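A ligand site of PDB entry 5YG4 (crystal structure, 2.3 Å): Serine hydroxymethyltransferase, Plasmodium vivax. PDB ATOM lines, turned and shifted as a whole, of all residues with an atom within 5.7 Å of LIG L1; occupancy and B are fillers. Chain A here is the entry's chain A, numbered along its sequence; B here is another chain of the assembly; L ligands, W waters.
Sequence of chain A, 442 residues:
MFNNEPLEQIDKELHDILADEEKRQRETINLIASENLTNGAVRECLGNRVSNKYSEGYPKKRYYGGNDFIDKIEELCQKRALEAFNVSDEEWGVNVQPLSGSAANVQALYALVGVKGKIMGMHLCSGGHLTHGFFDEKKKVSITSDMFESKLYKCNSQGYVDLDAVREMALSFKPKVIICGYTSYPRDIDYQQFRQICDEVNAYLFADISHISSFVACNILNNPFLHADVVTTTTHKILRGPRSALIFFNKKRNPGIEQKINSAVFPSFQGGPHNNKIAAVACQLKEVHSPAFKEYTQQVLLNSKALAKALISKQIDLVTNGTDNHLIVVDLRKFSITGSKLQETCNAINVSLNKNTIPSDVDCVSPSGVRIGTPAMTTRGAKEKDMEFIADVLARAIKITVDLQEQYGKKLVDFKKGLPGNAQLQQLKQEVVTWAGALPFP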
ATOM      1  N   ILE A  32     -13.410   5.147 -10.431  1.00  0.00           N
ATOM      2  CA  ILE A  32     -14.760   4.620 -10.766  1.00  0.00           C
ATOM      3  C   ILE A  32     -15.681   5.201  -9.721  1.00  0.00           C
ATOM      4  O   ILE A  32     -15.549   4.918  -8.535  1.00  0.00           O
ATOM      5  CB  ILE A  32     -14.886   3.080 -10.743  1.00  0.00           C
ATOM      6  CG1 ILE A  32     -13.934   2.397 -11.755  1.00  0.00           C
ATOM      7  CG2 ILE A  32     -16.321   2.680 -11.041  1.00  0.00           C
ATOM      8  CD1 ILE A  32     -14.198   2.667 -13.224  1.00  0.00           C
ATOM      9  N   SER A  34     -18.553   4.733  -8.796  1.00  0.00           N
ATOM     10  CA  SER A  34     -19.402   3.779  -8.094  1.00  0.00           C
ATOM     11  C   SER A  34     -18.678   2.777  -7.214  1.00  0.00           C
ATOM     12  O   SER A  34     -19.308   1.876  -6.724  1.00  0.00           O
ATOM     13  CB  SER A  34     -20.225   3.018  -9.136  1.00  0.00           C
ATOM     14  OG  SER A  34     -19.353   2.380 -10.079  1.00  0.00           O
ATOM     15  N   SER A 100     -28.835  -6.588  -4.173  1.00  0.00           N
ATOM     16  CA  SER A 100     -28.066  -5.544  -4.835  1.00  0.00           C
ATOM     17  C   SER A 100     -29.015  -4.446  -5.316  1.00  0.00           C
ATOM     18  O   SER A 100     -30.223  -4.608  -5.289  1.00  0.00           O
ATOM     19  CB  SER A 100     -27.249  -6.102  -6.034  1.00  0.00           C
ATOM     20  OG  SER A 100     -25.910  -5.565  -6.069  1.00  0.00           O
ATOM     21  N   GLY A 101     -28.488  -3.334  -5.806  1.00  0.00           N
ATOM     22  CA  GLY A 101     -29.325  -2.194  -6.168  1.00  0.00           C
ATOM     23  C   GLY A 101     -30.344  -2.415  -7.254  1.00  0.00           C
ATOM     24  O   GLY A 101     -31.416  -1.811  -7.248  1.00  0.00           O
ATOM     25  N   SER A 102     -29.991  -3.230  -8.231  1.00  0.00           N
ATOM     26  CA  SER A 102     -30.885  -3.496  -9.364  1.00  0.00           C
ATOM     27  C   SER A 102     -32.079  -4.321  -8.886  1.00  0.00           C
ATOM     28  O   SER A 102     -33.209  -4.009  -9.228  1.00  0.00           O
ATOM     29  CB  SER A 102     -30.145  -4.202 -10.523  1.00  0.00           C
ATOM     30  OG  SER A 102     -29.082  -3.414 -11.030  1.00  0.00           O
ATOM     31  N   ALA A 103     -31.829  -5.335  -8.065  1.00  0.00           N
ATOM     32  CA  ALA A 103     -32.902  -6.116  -7.452  1.00  0.00           C
ATOM     33  C   ALA A 103     -33.844  -5.221  -6.601  1.00  0.00           C
ATOM     34  O   ALA A 103     -35.039  -5.306  -6.727  1.00  0.00           O
ATOM     35  CB  ALA A 103     -32.327  -7.243  -6.614  1.00  0.00           C
ATOM     36  N   ASN A 105     -34.506  -2.038  -6.788  1.00  0.00           N
ATOM     37  CA  ASN A 105     -35.348  -1.218  -7.648  1.00  0.00           C
ATOM     38  C   ASN A 105     -36.447  -1.996  -8.375  1.00  0.00           C
ATOM     39  O   ASN A 105     -37.559  -1.530  -8.453  1.00  0.00           O
ATOM     40  CB  ASN A 105     -34.525  -0.463  -8.684  1.00  0.00           C
ATOM     41  CG  ASN A 105     -33.782   0.706  -8.090  1.00  0.00           C
ATOM     42  OD1 ASN A 105     -33.948   1.039  -6.914  1.00  0.00           O
ATOM     43  ND2 ASN A 105     -32.944   1.338  -8.911  1.00  0.00           N
ATOM     44  N   HIS A 129     -30.077   5.260 -14.496  1.00  0.00           N
ATOM     45  CA  HIS A 129     -29.686   3.851 -14.442  1.00  0.00           C
ATOM     46  C   HIS A 129     -30.566   2.983 -15.338  1.00  0.00           C
ATOM     47  O   HIS A 129     -31.676   3.370 -15.702  1.00  0.00           O
ATOM     48  CB  HIS A 129     -29.740   3.301 -13.006  1.00  0.00           C
ATOM     49  CG  HIS A 129     -28.933   2.052 -12.795  1.00  0.00           C
ATOM     50  ND1 HIS A 129     -29.500   0.816 -12.573  1.00  0.00           N
ATOM     51  CD2 HIS A 129     -27.594   1.841 -12.859  1.00  0.00           C
ATOM     52  CE1 HIS A 129     -28.542  -0.092 -12.477  1.00  0.00           C
ATOM     53  NE2 HIS A 129     -27.373   0.510 -12.649  1.00  0.00           N
ATOM     54  N   THR A 131     -32.136   0.317 -14.494  1.00  0.00           N
ATOM     55  CA  THR A 131     -33.353  -0.068 -13.760  1.00  0.00           C
ATOM     56  C   THR A 131     -34.377   1.054 -13.580  1.00  0.00           C
ATOM     57  O   THR A 131     -35.344   0.860 -12.855  1.00  0.00           O
ATOM     58  CB  THR A 131     -33.014  -0.594 -12.384  1.00  0.00           C
ATOM     59  OG1 THR A 131     -32.301   0.410 -11.648  1.00  0.00           O
ATOM     60  CG2 THR A 131     -32.206  -1.875 -12.520  1.00  0.00           C
ATOM     61  N   HIS A 132     -34.164   2.199 -14.240  1.00  0.00           N
ATOM     62  CA  HIS A 132     -35.127   3.298 -14.281  1.00  0.00           C
ATOM     63  C   HIS A 132     -35.949   3.257 -15.563  1.00  0.00           C
ATOM     64  O   HIS A 132     -36.476   4.275 -16.013  1.00  0.00           O
ATOM     65  CB  HIS A 132     -34.390   4.624 -14.149  1.00  0.00           C
ATOM     66  CG  HIS A 132     -33.607   4.773 -12.896  1.00  0.00           C
ATOM     67  ND1 HIS A 132     -32.813   5.867 -12.647  1.00  0.00           N
ATOM     68  CD2 HIS A 132     -33.480   3.969 -11.813  1.00  0.00           C
ATOM     69  CE1 HIS A 132     -32.240   5.736 -11.461  1.00  0.00           C
ATOM     70  NE2 HIS A 132     -32.633   4.594 -10.935  1.00  0.00           N
ATOM     71  N   GLY A 181     -32.834  10.547  -8.881  1.00  0.00           N
ATOM     72  CA  GLY A 181     -31.598  10.023  -8.280  1.00  0.00           C
ATOM     73  C   GLY A 181     -30.980   9.076  -9.297  1.00  0.00           C
ATOM     74  O   GLY A 181     -31.699   8.237  -9.894  1.00  0.00           O
ATOM     75  N   TYR A 182     -29.665   9.214  -9.524  1.00  0.00           N
ATOM     76  CA  TYR A 182     -29.081   8.819 -10.817  1.00  0.00           C
ATOM     77  C   TYR A 182     -27.712   8.186 -10.724  1.00  0.00           C
ATOM     78  O   TYR A 182     -27.099   8.126  -9.648  1.00  0.00           O
ATOM     79  CB  TYR A 182     -29.043  10.033 -11.737  1.00  0.00           C
ATOM     80  CG  TYR A 182     -30.356  10.834 -11.804  1.00  0.00           C
ATOM     81  CD1 TYR A 182     -31.540  10.281 -12.313  1.00  0.00           C
ATOM     82  CD2 TYR A 182     -30.411  12.175 -11.375  1.00  0.00           C
ATOM     83  CE1 TYR A 182     -32.720  11.008 -12.404  1.00  0.00           C
ATOM     84  CE2 TYR A 182     -31.592  12.917 -11.456  1.00  0.00           C
ATOM     85  CZ  TYR A 182     -32.742  12.338 -11.968  1.00  0.00           C
ATOM     86  OH  TYR A 182     -33.918  13.067 -12.051  1.00  0.00           O
ATOM     87  N   THR A 183     -27.240   7.657 -11.849  1.00  0.00           N
ATOM     88  CA  THR A 183     -25.939   6.945 -11.868  1.00  0.00           C
ATOM     89  C   THR A 183     -24.780   7.845 -12.270  1.00  0.00           C
ATOM     90  O   THR A 183     -23.709   7.699 -11.716  1.00  0.00           O
ATOM     91  CB  THR A 183     -25.903   5.657 -12.715  1.00  0.00           C
ATOM     92  OG1 THR A 183     -24.969   5.801 -13.812  1.00  0.00           O
ATOM     93  CG2 THR A 183     -27.176   5.304 -13.206  1.00  0.00           C
ATOM     94  N   ASP A 208     -33.645   7.185  -5.992  1.00  0.00           N
ATOM     95  CA  ASP A 208     -32.559   6.187  -5.939  1.00  0.00           C
ATOM     96  C   ASP A 208     -31.274   6.948  -5.659  1.00  0.00           C
ATOM     97  O   ASP A 208     -30.670   7.511  -6.588  1.00  0.00           O
ATOM     98  CB  ASP A 208     -32.453   5.419  -7.259  1.00  0.00           C
ATOM     99  CG  ASP A 208     -31.326   4.423  -7.284  1.00  0.00           C
ATOM    100  OD1 ASP A 208     -30.332   4.558  -6.536  1.00  0.00           O
ATOM    101  OD2 ASP A 208     -31.411   3.473  -8.082  1.00  0.00           O
ATOM    102  N   SER A 210     -28.331   5.808  -4.529  1.00  0.00           N
ATOM    103  CA  SER A 210     -27.168   4.906  -4.506  1.00  0.00           C
ATOM    104  C   SER A 210     -25.851   5.640  -4.648  1.00  0.00           C
ATOM    105  O   SER A 210     -24.930   5.383  -3.875  1.00  0.00           O
ATOM    106  CB  SER A 210     -27.291   3.834  -5.596  1.00  0.00           C
ATOM    107  OG  SER A 210     -28.541   3.130  -5.482  1.00  0.00           O
ATOM    108  N   HIS A 211     -25.787   6.573  -5.599  1.00  0.00           N
ATOM    109  CA  HIS A 211     -24.550   7.328  -5.839  1.00  0.00           C
ATOM    110  C   HIS A 211     -24.192   8.371  -4.787  1.00  0.00           C
ATOM    111  O   HIS A 211     -23.028   8.612  -4.541  1.00  0.00           O
ATOM    112  CB  HIS A 211     -24.480   7.913  -7.254  1.00  0.00           C
ATOM    113  CG  HIS A 211     -23.741   7.020  -8.205  1.00  0.00           C
ATOM    114  ND1 HIS A 211     -22.378   7.115  -8.405  1.00  0.00           N
ATOM    115  CD2 HIS A 211     -24.156   5.961  -8.917  1.00  0.00           C
ATOM    116  CE1 HIS A 211     -21.994   6.170  -9.232  1.00  0.00           C
ATOM    117  NE2 HIS A 211     -23.054   5.458  -9.567  1.00  0.00           N
ATOM    118  N   THR A 234     -28.092   1.418  -2.938  1.00  0.00           N
ATOM    119  CA  THR A 234     -27.050   0.449  -2.661  1.00  0.00           C
ATOM    120  C   THR A 234     -26.273   0.835  -1.416  1.00  0.00           C
ATOM    121  O   THR A 234     -26.277   1.979  -1.008  1.00  0.00           O
ATOM    122  CB  THR A 234     -26.053   0.326  -3.833  1.00  0.00           C
ATOM    123  OG1 THR A 234     -25.496   1.592  -4.144  1.00  0.00           O
ATOM    124  CG2 THR A 234     -26.756  -0.244  -5.067  1.00  0.00           C
ATOM    125  N   HIS A 236     -22.812  -0.225  -1.271  1.00  0.00           N
ATOM    126  CA  HIS A 236     -21.398  -0.457  -1.667  1.00  0.00           C
ATOM    127  C   HIS A 236     -20.663   0.710  -2.341  1.00  0.00           C
ATOM    128  O   HIS A 236     -19.449   0.593  -2.638  1.00  0.00           O
ATOM    129  CB  HIS A 236     -21.274  -1.690  -2.579  1.00  0.00           C
ATOM    130  CG  HIS A 236     -22.277  -1.770  -3.694  1.00  0.00           C
ATOM    131  ND1 HIS A 236     -23.552  -2.260  -3.517  1.00  0.00           N
ATOM    132  CD2 HIS A 236     -22.163  -1.495  -5.008  1.00  0.00           C
ATOM    133  CE1 HIS A 236     -24.191  -2.258  -4.661  1.00  0.00           C
ATOM    134  NE2 HIS A 236     -23.373  -1.801  -5.584  1.00  0.00           N
ATOM    135  N   LYS A 237     -21.349   1.816  -2.596  1.00  0.00           N
ATOM    136  CA  LYS A 237     -20.657   2.917  -3.283  1.00  0.00           C
ATOM    137  C   LYS A 237     -20.057   3.909  -2.259  1.00  0.00           C
ATOM    138  O   LYS A 237     -19.229   3.519  -1.419  1.00  0.00           O
ATOM    139  CB  LYS A 237     -21.571   3.567  -4.286  1.00  0.00           C
ATOM    140  CG  LYS A 237     -22.177   2.625  -5.303  1.00  0.00           C
ATOM    141  CD  LYS A 237     -23.111   3.437  -6.193  1.00  0.00           C
ATOM    142  CE  LYS A 237     -23.707   2.607  -7.299  1.00  0.00           C
ATOM    143  NZ  LYS A 237     -24.290   1.348  -6.805  1.00  0.00           N
ATOM    144  N   ARG A 243     -21.838  -5.261  -0.868  1.00  0.00           N
ATOM    145  CA  ARG A 243     -22.690  -5.168  -2.029  1.00  0.00           C
ATOM    146  C   ARG A 243     -24.057  -5.646  -1.601  1.00  0.00           C
ATOM    147  O   ARG A 243     -24.270  -6.825  -1.425  1.00  0.00           O
ATOM    148  CB  ARG A 243     -22.163  -5.960  -3.225  1.00  0.00           C
ATOM    149  CG  ARG A 243     -20.772  -5.556  -3.643  1.00  0.00           C
ATOM    150  CD  ARG A 243     -20.351  -6.224  -4.960  1.00  0.00           C
ATOM    151  NE  ARG A 243     -20.747  -5.420  -6.095  1.00  0.00           N
ATOM    152  CZ  ARG A 243     -20.081  -4.366  -6.558  1.00  0.00           C
ATOM    153  NH1 ARG A 243     -18.931  -3.953  -6.034  1.00  0.00           N
ATOM    154  NH2 ARG A 243     -20.587  -3.717  -7.580  1.00  0.00           N
ATOM    155  N   SER A 244     -24.967  -4.687  -1.400  1.00  0.00           N
ATOM    156  CA  SER A 244     -26.307  -4.970  -0.935  1.00  0.00           C
ATOM    157  C   SER A 244     -27.178  -3.763  -1.210  1.00  0.00           C
ATOM    158  O   SER A 244     -26.698  -2.756  -1.729  1.00  0.00           O
ATOM    159  CB  SER A 244     -26.306  -5.257   0.571  1.00  0.00           C
ATOM    160  OG  SER A 244     -27.406  -6.074   0.919  1.00  0.00           O
ATOM    161  N   ARG A 371     -16.569   9.313 -16.936  1.00  0.00           N
ATOM    162  CA  ARG A 371     -17.018   9.664 -15.615  1.00  0.00           C
ATOM    163  C   ARG A 371     -15.916   9.347 -14.610  1.00  0.00           C
ATOM    164  O   ARG A 371     -15.301   8.282 -14.676  1.00  0.00           O
ATOM    165  CB  ARG A 371     -18.274   8.884 -15.305  1.00  0.00           C
ATOM    166  CG  ARG A 371     -18.990   9.287 -14.046  1.00  0.00           C
ATOM    167  CD  ARG A 371     -20.049   8.251 -13.689  1.00  0.00           C
ATOM    168  NE  ARG A 371     -19.478   6.972 -13.224  1.00  0.00           N
ATOM    169  CZ  ARG A 371     -20.202   5.903 -12.900  1.00  0.00           C
ATOM    170  NH1 ARG A 371     -21.525   5.937 -12.966  1.00  0.00           N
ATOM    171  NH2 ARG A 371     -19.605   4.792 -12.507  1.00  0.00           N
ATOM    172  N   TYR B  54     -16.475  -3.233  -9.585  1.00  0.00           N
ATOM    173  CA  TYR B  54     -17.613  -3.209 -10.496  1.00  0.00           C
ATOM    174  C   TYR B  54     -17.108  -3.803 -11.800  1.00  0.00           C
ATOM    175  O   TYR B  54     -16.081  -3.370 -12.328  1.00  0.00           O
ATOM    176  CB  TYR B  54     -18.186  -1.796 -10.717  1.00  0.00           C
ATOM    177  CG  TYR B  54     -19.569  -1.606 -10.115  1.00  0.00           C
ATOM    178  CD1 TYR B  54     -20.664  -2.269 -10.644  1.00  0.00           C
ATOM    179  CD2 TYR B  54     -19.778  -0.752  -9.026  1.00  0.00           C
ATOM    180  CE1 TYR B  54     -21.922  -2.116 -10.102  1.00  0.00           C
ATOM    181  CE2 TYR B  54     -21.040  -0.593  -8.471  1.00  0.00           C
ATOM    182  CZ  TYR B  54     -22.113  -1.279  -9.007  1.00  0.00           C
ATOM    183  OH  TYR B  54     -23.372  -1.140  -8.474  1.00  0.00           O
ATOM    184  N   GLU B  56     -19.455  -5.022 -14.631  1.00  0.00           N
ATOM    185  CA  GLU B  56     -20.655  -5.293 -15.422  1.00  0.00           C
ATOM    186  C   GLU B  56     -20.315  -5.792 -16.802  1.00  0.00           C
ATOM    187  O   GLU B  56     -19.377  -5.312 -17.426  1.00  0.00           O
ATOM    188  CB  GLU B  56     -21.475  -4.037 -15.561  1.00  0.00           C
ATOM    189  CG  GLU B  56     -22.041  -3.614 -14.235  1.00  0.00           C
ATOM    190  CD  GLU B  56     -22.923  -2.416 -14.356  1.00  0.00           C
ATOM    191  OE1 GLU B  56     -22.406  -1.357 -14.719  1.00  0.00           O
ATOM    192  OE2 GLU B  56     -24.108  -2.557 -14.082  1.00  0.00           O
ATOM    193  N   TYR B  64     -16.366  -1.919 -18.261  1.00  0.00           N
ATOM    194  CA  TYR B  64     -15.239  -1.256 -17.601  1.00  0.00           C
ATOM    195  C   TYR B  64     -13.990  -2.060 -17.842  1.00  0.00           C
ATOM    196  O   TYR B  64     -14.054  -3.229 -18.176  1.00  0.00           O
ATOM    197  CB  TYR B  64     -15.447  -1.219 -16.089  1.00  0.00           C
ATOM    198  CG  TYR B  64     -16.547  -0.327 -15.621  1.00  0.00           C
ATOM    199  CD1 TYR B  64     -17.385   0.330 -16.516  1.00  0.00           C
ATOM    200  CD2 TYR B  64     -16.745  -0.139 -14.249  1.00  0.00           C
ATOM    201  CE1 TYR B  64     -18.388   1.143 -16.064  1.00  0.00           C
ATOM    202  CE2 TYR B  64     -17.756   0.693 -13.784  1.00  0.00           C
ATOM    203  CZ  TYR B  64     -18.583   1.341 -14.696  1.00  0.00           C
ATOM    204  OH  TYR B  64     -19.596   2.159 -14.273  1.00  0.00           O
ATOM    205  N   GLN B 270     -29.837  -7.963 -13.410  1.00  0.00           N
ATOM    206  CA  GLN B 270     -28.816  -7.550 -12.455  1.00  0.00           C
ATOM    207  C   GLN B 270     -27.942  -6.421 -13.014  1.00  0.00           C
ATOM    208  O   GLN B 270     -28.040  -6.082 -14.193  1.00  0.00           O
ATOM    209  CB  GLN B 270     -27.950  -8.741 -12.043  1.00  0.00           C
ATOM    210  CG  GLN B 270     -28.724  -9.904 -11.464  1.00  0.00           C
ATOM    211  CD  GLN B 270     -27.844 -11.022 -10.865  1.00  0.00           C
ATOM    212  OE1 GLN B 270     -28.355 -11.890 -10.145  1.00  0.00           O
ATOM    213  NE2 GLN B 270     -26.540 -11.027 -11.157  1.00  0.00           N
ATOM    214  N   GLY B 271     -27.134  -5.838 -12.142  1.00  0.00           N
ATOM    215  CA  GLY B 271     -26.112  -4.869 -12.472  1.00  0.00           C
ATOM    216  C   GLY B 271     -24.752  -5.518 -12.212  1.00  0.00           C
ATOM    217  O   GLY B 271     -24.417  -6.548 -12.820  1.00  0.00           O
ATOM    218  N   GLY B 272     -23.966  -4.945 -11.294  1.00  0.00           N
ATOM    219  CA  GLY B 272     -22.592  -5.430 -11.099  1.00  0.00           C
ATOM    220  C   GLY B 272     -22.560  -6.811 -10.476  1.00  0.00           C
ATOM    221  O   GLY B 272     -23.295  -7.053  -9.525  1.00  0.00           O
ATOM    222  N   HIS B 274     -21.216  -9.973  -8.158  1.00  0.00           N
ATOM    223  CA  HIS B 274     -20.618 -10.039  -6.857  1.00  0.00           C
ATOM    224  C   HIS B 274     -19.473 -11.003  -6.964  1.00  0.00           C
ATOM    225  O   HIS B 274     -19.649 -12.238  -6.969  1.00  0.00           O
ATOM    226  CB  HIS B 274     -21.644 -10.467  -5.831  1.00  0.00           C
ATOM    227  CG  HIS B 274     -22.682  -9.421  -5.530  1.00  0.00           C
ATOM    228  ND1 HIS B 274     -23.404  -9.420  -4.359  1.00  0.00           N
ATOM    229  CD2 HIS B 274     -23.099  -8.327  -6.219  1.00  0.00           C
ATOM    230  CE1 HIS B 274     -24.238  -8.398  -4.343  1.00  0.00           C
ATOM    231  NE2 HIS B 274     -24.068  -7.715  -5.460  1.00  0.00           N
HETATM  232  N1  LIG L   1     -28.930   2.642  -8.891  1.00  0.00           N
HETATM  233  C1  LIG L   1     -28.047   3.538  -9.331  1.00  0.00           C
HETATM  234  C2  LIG L   1     -28.439   4.999  -9.369  1.00  0.00           C
HETATM  235  C3  LIG L   1     -26.737   3.062  -9.763  1.00  0.00           C
HETATM  236  O1  LIG L   1     -25.850   3.952 -10.215  1.00  0.00           O
HETATM  237  C4  LIG L   1     -26.419   1.621  -9.724  1.00  0.00           C
HETATM  238  C5  LIG L   1     -25.041   1.093 -10.161  1.00  0.00           C
HETATM  239  C6  LIG L   1     -27.515   0.739  -9.198  1.00  0.00           C
HETATM  240  C7  LIG L   1     -28.711   1.324  -8.841  1.00  0.00           C
HETATM  241  C8  LIG L   1     -27.474  -0.754  -9.109  1.00  0.00           C
HETATM  242  O2  LIG L   1     -26.480  -1.333  -8.294  1.00  0.00           O
HETATM  243  P1  LIG L   1     -26.165  -2.893  -8.498  1.00  0.00           P
HETATM  244  O3  LIG L   1     -27.381  -3.615  -8.978  1.00  0.00           O
HETATM  245  O4  LIG L   1     -25.092  -2.867  -9.549  1.00  0.00           O
HETATM  246  O5  LIG L   1     -25.654  -3.231  -7.136  1.00  0.00           O
HETATM  247  C9  LIG L   1     -22.275   2.165 -11.811  1.00  0.00           C
HETATM  248  O6  LIG L   1     -21.115   1.762 -11.789  1.00  0.00           O
HETATM  249  O7  LIG L   1     -22.519   3.392 -11.665  1.00  0.00           O
HETATM  250  C10 LIG L   1     -23.346   1.079 -12.031  1.00  0.00           C
HETATM  251  N2  LIG L   1     -24.622   1.495 -11.471  1.00  0.00           N
HETATM  252  C1  LG2 L   2     -25.325   4.942 -16.982  1.00  0.00           C
HETATM  253  C2  LG2 L   2     -24.343   4.480 -17.814  1.00  0.00           C
HETATM  254  C3  LG2 L   2     -23.775   3.060 -17.623  1.00  0.00           C
HETATM  255  C4  LG2 L   2     -24.761   2.171 -16.927  1.00  0.00           C
HETATM  256  C5  LG2 L   2     -25.834   2.722 -16.106  1.00  0.00           C
HETATM  257  N1  LG2 L   2     -25.873   6.148 -17.050  1.00  0.00           N
HETATM  258  C6  LG2 L   2     -23.831   5.236 -18.722  1.00  0.00           C
HETATM  259  C7  LG2 L   2     -25.026   0.691 -16.794  1.00  0.00           C
HETATM  260  C8  LG2 L   2     -24.322  -0.526 -17.385  1.00  0.00           C
HETATM  261  C9  LG2 L   2     -21.929   1.868 -16.188  1.00  0.00           C
HETATM  262  C10 LG2 L   2     -23.475   2.440 -18.942  1.00  0.00           C
HETATM  263  C11 LG2 L   2     -22.157   2.598 -19.241  1.00  0.00           C
HETATM  264  C12 LG2 L   2     -21.644   2.114 -20.416  1.00  0.00           C
HETATM  265  C13 LG2 L   2     -24.367   1.799 -19.818  1.00  0.00           C
HETATM  266  O1  LG2 L   2     -26.400  -3.024 -26.084  1.00  0.00           O
HETATM  267  C14 LG2 L   2     -26.999  -3.114 -24.964  1.00  0.00           C
HETATM  268  O2  LG2 L   2     -27.315  -4.230 -24.436  1.00  0.00           O
HETATM  269  C15 LG2 L   2     -27.373  -1.802 -24.274  1.00  0.00           C
HETATM  270  C16 LG2 L   2     -26.220  -1.112 -23.507  1.00  0.00           C
HETATM  271  C17 LG2 L   2     -25.891   0.264 -24.056  1.00  0.00           C
HETATM  272  C18 LG2 L   2     -24.620   0.794 -23.350  1.00  0.00           C
HETATM  273  C19 LG2 L   2     -26.616  -0.979 -22.069  1.00  0.00           C
HETATM  274  C20 LG2 L   2     -25.407  -0.586 -21.244  1.00  0.00           C
HETATM  275  N2  LG2 L   2     -24.702   0.541 -21.907  1.00  0.00           N
HETATM  276  C21 LG2 L   2     -23.884   1.291 -21.031  1.00  0.00           C
HETATM  277  C22 LG2 L   2     -22.512   1.459 -21.303  1.00  0.00           C
HETATM  278  F1  LG2 L   2     -20.337   2.289 -20.679  1.00  0.00           F
HETATM  279  C23 LG2 L   2     -21.412   3.338 -18.155  1.00  0.00           C
HETATM  280  C24 LG2 L   2     -22.357   3.148 -16.942  1.00  0.00           C
HETATM  281  C25 LG2 L   2     -22.163   4.315 -15.948  1.00  0.00           C
HETATM  282  N3  LG2 L   2     -23.373   5.939 -19.549  1.00  0.00           N
HETATM  283  N4  LG2 L   2     -26.114   0.601 -15.976  1.00  0.00           N
HETATM  284  N5  LG2 L   2     -26.645   1.825 -15.556  1.00  0.00           N
HETATM  285  O3  LG2 L   2     -25.904   4.070 -15.966  1.00  0.00           O
HETATM  286  O   HOH W   1     -25.289  -1.429 -12.037  1.00  0.00           O
HETATM  287  O   HOH W   2     -26.934  -6.556  -9.474  1.00  0.00           O
HETATM  288  O   HOH W   3     -23.064  -4.960  -7.534  1.00  0.00           O
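O5 of LIG L1 lies close to NE2 of His 236, at 3.1 Å. The side-chain hydroxyl (OG) of Ser 102 sits at hydrogen-bond distance from an oxygen (O3) of LIG L1 (2.7 Å). OD2 of Asp 208 lies within hydrogen-bond range of N1 of LIG L1, 2.7 Å away. N of Gly 272 of chain B is in hydrogen-bond range of O4 of LIG L1 (2.9 Å). O5 of LIG L1 is in hydrogen-bond range of N of Gly 101 (3.1 Å). O6 of LIG L1 is in hydrogen-bond range of OG of Ser 34 (2.5 Å). NE2 of His 211 is in hydrogen-bond range of O7 of LIG L1 (3.0 Å). N5 of LG2 L2 lies close to NE2 of His 129, 3.3 Å away. An oxygen (O5) of LIG L1 is in hydrogen-bond range of the side-chain hydroxyl (OG) of Ser 100. OH of Tyr 64 of chain B sits at hydrogen-bond distance from O6 of LIG L1 (2.9 Å). The side-chain hydroxyl (OG) of Ser 210 is in hydrogen-bond range of a nitrogen (N1) of LIG L1, at 3.5 Å. A ring nitrogen (NE2) of His 129 lies within hydrogen-bond range of a nitrogen (N2) of LIG L1, at 3.2 Å. An oxygen (O4) of LIG L1 sits at hydrogen-bond distance from the side-chain hydroxyl (OH) of Tyr 54 of chain B (2.7 Å). An oxygen (O7) of LIG L1 lies within salt-bridge range of the guanidinium group (NH1) of Arg 371 (3.0 Å). The backbone NH (N) of Ser 102 is in hydrogen-bond range of an oxygen (O3) of LIG L1 (2.7 Å). The side-chain hydroxyl (OG1) of Thr 183 sits at hydrogen-bond distance from an oxygen (O3) of LG2 L2 (2.9 Å).
A ring nitrogen (NE2) of His 236 is in hydrogen-bond range of the side-chain amino group (NZ) of Lys 237 (3.5 Å). A ring nitrogen (NE2) of His 132 is in hydrogen-bond range of the side-chain carboxylate (OD2) of Asp 208, at 3.3 Å. The guanidinium group of Arg 371 sits at hydrogen-bond distance from the backbone carbonyl oxygen of Thr 183 (3.1 Å). NE2 of His 274 of chain B is in hydrogen-bond range of OG of Ser 100. NH2 of Arg 371 is in hydrogen-bond range of OG of Ser 34. OG of Ser 210 is in hydrogen-bond range of N of Thr 234, at 3.1 Å. NZ of Lys 237 lies within hydrogen-bond range of OH of Tyr 54 of chain B (3.1 Å). The side-chain carboxylate (OD1) of Asp 208 lies within hydrogen-bond range of the side-chain hydroxyl (OG) of Ser 210 (2.5 Å).
Water W1 lies within hydrogen-bond range of the side-chain carboxylate of Glu 56 of chain B (2.6 Å), an oxygen (O4) of LIG L1 (2.9 Å) and a ring nitrogen (NE2) of His 129 (2.9 Å). Water W2 lies within hydrogen-bond range of the backbone NH of Gly 271 of chain B (2.8 Å) and an oxygen (O3) of LIG L1 (3.0 Å). Water W3 lies within hydrogen-bond range of the guanidinium group of Arg 243 (2.8 Å), the backbone carbonyl oxygen of Gly 272 of chain B (2.9 Å), an oxygen (O5) of LIG L1 (3.1 Å) and the side-chain hydroxyl of Ser 100 (3.3 Å).
Tyr 182 touches LIG L1 (O to C2, 3.4 Å). Thr 183 touches LIG L1 (CB to O1, 3.0 Å). CG2 of Thr 234 touches O2 of LIG L1 (3.4 Å). Lys 237 touches LIG L1 (NZ to C5, 3.4 Å). OE1 of Glu 56 of chain B touches C10 of LIG L1 (3.7 Å). Gly 271 of chain B touches LIG L1. Hydrophobic or aromatic side chains within 4 Å of LIG L1: His 129, His 211, His 236, Tyr 54 of chain B and Tyr 64 of chain B. Of the 29 residues printed, 19 come within 4 Å of LIG L1.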
